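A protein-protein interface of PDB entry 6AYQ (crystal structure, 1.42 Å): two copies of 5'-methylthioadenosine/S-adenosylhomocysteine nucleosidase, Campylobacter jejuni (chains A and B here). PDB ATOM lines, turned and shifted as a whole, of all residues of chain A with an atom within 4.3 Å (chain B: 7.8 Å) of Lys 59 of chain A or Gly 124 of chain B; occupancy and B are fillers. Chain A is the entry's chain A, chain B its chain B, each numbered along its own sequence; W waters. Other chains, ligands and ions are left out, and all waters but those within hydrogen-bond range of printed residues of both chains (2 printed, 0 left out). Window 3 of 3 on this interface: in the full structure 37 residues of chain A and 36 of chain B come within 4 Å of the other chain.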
ATOM      1  N   ALA A  18      13.371   1.012  -6.378  1.00  0.00           N
ATOM      2  CA  ALA A  18      13.166   0.279  -5.128  1.00  0.00           C
ATOM      3  C   ALA A  18      11.765   0.429  -4.584  1.00  0.00           C
ATOM      4  O   ALA A  18      11.200  -0.545  -4.097  1.00  0.00           O
ATOM      5  CB  ALA A  18      14.169   0.717  -4.072  1.00  0.00           C
ATOM      6  N   ASN A  40       6.952 -12.689  -5.828  1.00  0.00           N
ATOM      7  CA  ASN A  40       6.264 -11.931  -4.777  1.00  0.00           C
ATOM      8  C   ASN A  40       6.281 -10.421  -5.048  1.00  0.00           C
ATOM      9  O   ASN A  40       6.586  -9.604  -4.178  1.00  0.00           O
ATOM     10  CB  ASN A  40       6.854 -12.269  -3.398  1.00  0.00           C
ATOM     11  CG  ASN A  40       5.957 -11.836  -2.250  1.00  0.00           C
ATOM     12  OD1 ASN A  40       4.731 -11.765  -2.389  1.00  0.00           O
ATOM     13  ND2 ASN A  40       6.567 -11.539  -1.103  1.00  0.00           N
ATOM     14  N   ASN A  41       5.956 -10.064  -6.285  1.00  0.00           N
ATOM     15  CA  ASN A  41       6.037  -8.682  -6.745  1.00  0.00           C
ATOM     16  C   ASN A  41       5.257  -8.570  -8.050  1.00  0.00           C
ATOM     17  O   ASN A  41       4.782  -9.573  -8.585  1.00  0.00           O
ATOM     18  CB  ASN A  41       7.512  -8.312  -6.969  1.00  0.00           C
ATOM     19  CG  ASN A  41       7.796  -6.827  -6.815  1.00  0.00           C
ATOM     20  OD1 ASN A  41       6.909  -5.974  -6.860  1.00  0.00           O
ATOM     21  ND2 ASN A  41       9.071  -6.512  -6.637  1.00  0.00           N
ATOM     22  N   TYR A  57       9.289  -1.972  -9.186  1.00  0.00           N
ATOM     23  CA  TYR A  57       9.999  -1.550  -7.978  1.00  0.00           C
ATOM     24  C   TYR A  57      10.264  -2.807  -7.151  1.00  0.00           C
ATOM     25  O   TYR A  57       9.393  -3.665  -6.984  1.00  0.00           O
ATOM     26  CB  TYR A  57       9.275  -0.440  -7.212  1.00  0.00           C
ATOM     27  CG  TYR A  57       7.940  -0.792  -6.639  1.00  0.00           C
ATOM     28  CD1 TYR A  57       7.842  -1.402  -5.385  1.00  0.00           C
ATOM     29  CD2 TYR A  57       6.777  -0.481  -7.313  1.00  0.00           C
ATOM     30  CE1 TYR A  57       6.610  -1.719  -4.838  1.00  0.00           C
ATOM     31  CE2 TYR A  57       5.533  -0.773  -6.767  1.00  0.00           C
ATOM     32  CZ  TYR A  57       5.460  -1.399  -5.537  1.00  0.00           C
ATOM     33  OH  TYR A  57       4.237  -1.706  -4.980  1.00  0.00           O
ATOM     34  N   SER A  58      11.500  -2.934  -6.686  1.00  0.00           N
ATOM     35  CA  SER A  58      11.972  -4.181  -6.079  1.00  0.00           C
ATOM     36  C   SER A  58      11.524  -4.426  -4.642  1.00  0.00           C
ATOM     37  O   SER A  58      11.559  -5.580  -4.185  1.00  0.00           O
ATOM     38  CB  SER A  58      13.507  -4.199  -6.106  1.00  0.00           C
ATOM     39  OG  SER A  58      14.078  -3.106  -5.412  1.00  0.00           O
ATOM     40  N   LYS A  59      11.117  -3.359  -3.956  1.00  0.00           N
ATOM     41  CA  LYS A  59      11.104  -3.241  -2.503  1.00  0.00           C
ATOM     42  C   LYS A  59      12.522  -2.946  -2.017  1.00  0.00           C
ATOM     43  O   LYS A  59      13.514  -3.116  -2.738  1.00  0.00           O
ATOM     44  CB  LYS A  59      10.441  -4.414  -1.780  1.00  0.00           C
ATOM     45  CG  LYS A  59       8.997  -4.630  -2.225  1.00  0.00           C
ATOM     46  CD  LYS A  59       8.406  -5.907  -1.656  1.00  0.00           C
ATOM     47  CE  LYS A  59       8.868  -7.123  -2.432  1.00  0.00           C
ATOM     48  NZ  LYS A  59       8.291  -8.394  -1.915  1.00  0.00           N
ATOM     49  N   ILE A  60      12.602  -2.415  -0.811  1.00  0.00           N
ATOM     50  CA  ILE A  60      13.833  -1.794  -0.331  1.00  0.00           C
ATOM     51  C   ILE A  60      14.953  -2.800  -0.068  1.00  0.00           C
ATOM     52  O   ILE A  60      14.740  -3.878   0.487  1.00  0.00           O
ATOM     53  CB  ILE A  60      13.534  -0.980   0.945  1.00  0.00           C
ATOM     54  CG1 ILE A  60      12.681   0.247   0.578  1.00  0.00           C
ATOM     55  CG2 ILE A  60      14.816  -0.546   1.649  1.00  0.00           C
ATOM     56  CD1 ILE A  60      11.994   0.880   1.764  1.00  0.00           C
ATOM     57  N   GLY A  61      16.177  -2.412  -0.453  1.00  0.00           N
ATOM     58  CA  GLY A  61      17.383  -3.092   0.017  1.00  0.00           C
ATOM     59  C   GLY A  61      18.067  -4.012  -0.968  1.00  0.00           C
ATOM     60  O   GLY A  61      17.609  -4.240  -2.092  1.00  0.00           O
ATOM     61  N   ASN A  64      16.218  -7.633  -2.003  1.00  0.00           N
ATOM     62  CA  ASN A  64      15.074  -7.391  -2.887  1.00  0.00           C
ATOM     63  C   ASN A  64      15.492  -6.907  -4.272  1.00  0.00           C
ATOM     64  O   ASN A  64      14.966  -7.382  -5.292  1.00  0.00           O
ATOM     65  CB  ASN A  64      14.116  -6.380  -2.265  1.00  0.00           C
ATOM     66  CG  ASN A  64      13.286  -6.956  -1.120  1.00  0.00           C
ATOM     67  OD1 ASN A  64      12.883  -8.133  -1.131  1.00  0.00           O
ATOM     68  ND2 ASN A  64      13.048  -6.131  -0.105  1.00  0.00           N
ATOM     69  N   PHE B 121      12.936  -5.308   9.120  1.00  0.00           N
ATOM     70  CA  PHE B 121      11.703  -5.141   8.366  1.00  0.00           C
ATOM     71  C   PHE B 121      11.820  -4.107   7.250  1.00  0.00           C
ATOM     72  O   PHE B 121      12.327  -3.019   7.476  1.00  0.00           O
ATOM     73  CB  PHE B 121      10.567  -4.710   9.317  1.00  0.00           C
ATOM     74  CG  PHE B 121       9.240  -4.537   8.618  1.00  0.00           C
ATOM     75  CD1 PHE B 121       8.371  -5.609   8.483  1.00  0.00           C
ATOM     76  CD2 PHE B 121       8.881  -3.315   8.071  1.00  0.00           C
ATOM     77  CE1 PHE B 121       7.171  -5.469   7.797  1.00  0.00           C
ATOM     78  CE2 PHE B 121       7.683  -3.172   7.387  1.00  0.00           C
ATOM     79  CZ  PHE B 121       6.829  -4.238   7.267  1.00  0.00           C
ATOM     80  N   VAL B 122      11.348  -4.471   6.054  1.00  0.00           N
ATOM     81  CA  VAL B 122      10.979  -3.486   5.031  1.00  0.00           C
ATOM     82  C   VAL B 122       9.555  -3.751   4.511  1.00  0.00           C
ATOM     83  O   VAL B 122       9.119  -4.916   4.447  1.00  0.00           O
ATOM     84  CB  VAL B 122      11.959  -3.436   3.830  1.00  0.00           C
ATOM     85  CG1 VAL B 122      13.343  -3.038   4.307  1.00  0.00           C
ATOM     86  CG2 VAL B 122      12.002  -4.749   3.063  1.00  0.00           C
ATOM     87  N   PRO B 123       8.856  -2.681   4.083  1.00  0.00           N
ATOM     88  CA  PRO B 123       7.469  -2.859   3.630  1.00  0.00           C
ATOM     89  C   PRO B 123       7.335  -3.869   2.512  1.00  0.00           C
ATOM     90  O   PRO B 123       8.155  -3.886   1.599  1.00  0.00           O
ATOM     91  CB  PRO B 123       7.094  -1.478   3.134  1.00  0.00           C
ATOM     92  CG  PRO B 123       7.886  -0.559   3.974  1.00  0.00           C
ATOM     93  CD  PRO B 123       9.193  -1.256   4.243  1.00  0.00           C
ATOM     94  N   GLY B 124       6.300  -4.709   2.592  1.00  0.00           N
ATOM     95  CA  GLY B 124       6.068  -5.724   1.582  1.00  0.00           C
ATOM     96  C   GLY B 124       6.597  -7.089   1.970  1.00  0.00           C
ATOM     97  O   GLY B 124       6.165  -8.099   1.408  1.00  0.00           O
ATOM     98  N   ASN B 125       7.554  -7.125   2.904  1.00  0.00           N
ATOM     99  CA  ASN B 125       8.160  -8.355   3.404  1.00  0.00           C
ATOM    100  C   ASN B 125       7.850  -8.480   4.903  1.00  0.00           C
ATOM    101  O   ASN B 125       7.135  -7.669   5.459  1.00  0.00           O
ATOM    102  CB  ASN B 125       9.678  -8.300   3.148  1.00  0.00           C
ATOM    103  CG  ASN B 125      10.042  -8.380   1.664  1.00  0.00           C
ATOM    104  OD1 ASN B 125       9.172  -8.372   0.784  1.00  0.00           O
ATOM    105  ND2 ASN B 125      11.340  -8.452   1.378  1.00  0.00           N
ATOM    106  N   GLU B 126       8.367  -9.511   5.553  1.00  0.00           N
ATOM    107  CA  GLU B 126       8.220  -9.664   6.994  1.00  0.00           C
ATOM    108  C   GLU B 126       9.598  -9.721   7.621  1.00  0.00           C
ATOM    109  O   GLU B 126      10.607  -9.845   6.909  1.00  0.00           O
ATOM    110  CB  GLU B 126       7.444 -10.935   7.315  1.00  0.00           C
ATOM    111  CG  GLU B 126       5.977 -10.868   6.932  1.00  0.00           C
ATOM    112  CD  GLU B 126       5.246 -12.135   7.310  1.00  0.00           C
ATOM    113  OE1 GLU B 126       5.489 -13.184   6.669  1.00  0.00           O
ATOM    114  OE2 GLU B 126       4.422 -12.088   8.242  1.00  0.00           O
ATOM    115  N   LEU B 189      14.335 -16.215   1.260  1.00  0.00           N
ATOM    116  CA  LEU B 189      13.465 -15.204   0.651  1.00  0.00           C
ATOM    117  C   LEU B 189      13.276 -15.448  -0.839  1.00  0.00           C
ATOM    118  O   LEU B 189      12.129 -15.409  -1.328  1.00  0.00           O
ATOM    119  CB  LEU B 189      14.036 -13.810   0.900  1.00  0.00           C
ATOM    120  CG  LEU B 189      13.202 -12.603   0.458  1.00  0.00           C
ATOM    121  CD1 LEU B 189      13.528 -11.394   1.325  1.00  0.00           C
ATOM    122  CD2 LEU B 189      13.401 -12.270  -1.022  1.00  0.00           C
ATOM    123  N   ALA B 193       9.741 -16.500  -2.614  1.00  0.00           N
ATOM    124  CA  ALA B 193       9.213 -15.623  -3.651  1.00  0.00           C
ATOM    125  C   ALA B 193       8.939 -16.380  -4.950  1.00  0.00           C
ATOM    126  O   ALA B 193       7.955 -16.078  -5.639  1.00  0.00           O
ATOM    127  CB  ALA B 193      10.178 -14.473  -3.897  1.00  0.00           C
HETATM  128  O   HOH W   1      10.178  -2.072   0.796  1.00  0.00           O
HETATM  129  O   HOH W   2       5.521  -8.101  -1.600  1.00  0.00           O
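No position is printed for both chains.
Of the 7 pairs that touch across the chains among the printed residues, none has its exchanged pair printed and touching as well.
O of Asn 40 of chain A sits at hydrogen-bond distance from NZ of Lys 59 of chain A, 3.1 Å away.
The backbone carbonyl oxygen (O) of Ala 18 of chain A sits at hydrogen-bond distance from the backbone NH (N) of Lys 59 of chain A.
O of Ile 60 of chain A is in hydrogen-bond range of ND2 of Asn 64 of chain A (2.9 Å).
Of the 9 printed residues of chain A, 4 touch a printed residue of chain B.
Hydrophobic or aromatic side chains of chain A within 4 Å of the printed part of chain B: Ile 60.
Hydrophobic or aromatic side chains of chain B within 4 Å of the printed part of chain A: Val 122.
Along chain B the printed residues that touch a printed residue of chain A span positions 122 to 193.
Among the printed residues, 7 pairs touch across the chains.
Among the printed residues, no Asp or Glu carboxylate lies within 4 Å of a Lys or Arg side-chain nitrogen of the other chain.
Water W2 lies within hydrogen-bond range of NZ of Lys 59 of chain A, O of Gly 124 of chain B and O of Asn 40 of chain A.
Water W1 lies within hydrogen-bond range of O of Pro 123 of chain B (2.8 Å) and N of Ile 60 of chain A (2.9 Å).
The side-chain amide nitrogen (ND2) of Asn 125 of chain B sits at hydrogen-bond distance from the side-chain amide oxygen (OD1) of Asn 64 of chain A, at 3.0 Å.
NZ of Lys 59 of chain A is in hydrogen-bond range of OD1 of Asn 125 of chain B.
Lys 59 of chain A touches three residues of chain B.
Of the printed residues of chain A, Gly 124 of chain B touches Lys 59.
Of the printed residues of chain A, Pro 123 of chain B touches Lys 59.
Of the printed residues of chain B, Ile 60 of chain A touches Val 122 (3.9 Å).
Printed residues of chain A within 4 Å of Ala 193 of chain B: Asn 40 (3.5 Å).
Ala 18 of chain A touches none of the printed residues of chain B.
The nearest residue of chain B that does not touch Lys 59 of chain A is Val 122 of chain B (5.1 Å).
Among the printed residues, merely in contact across the chains: Asn 40 of chain A with Ala 193 of chain B (3.5 Å), Lys 59 of chain A with Pro 123 of chain B (3.8 Å), Lys 59 of chain A with Gly 124 of chain B (3.96 Å), Ile 60 of chain A with Val 122 of chain B (3.9 Å) and Asn 64 of chain A with Val 122 of chain B (3.6 Å).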
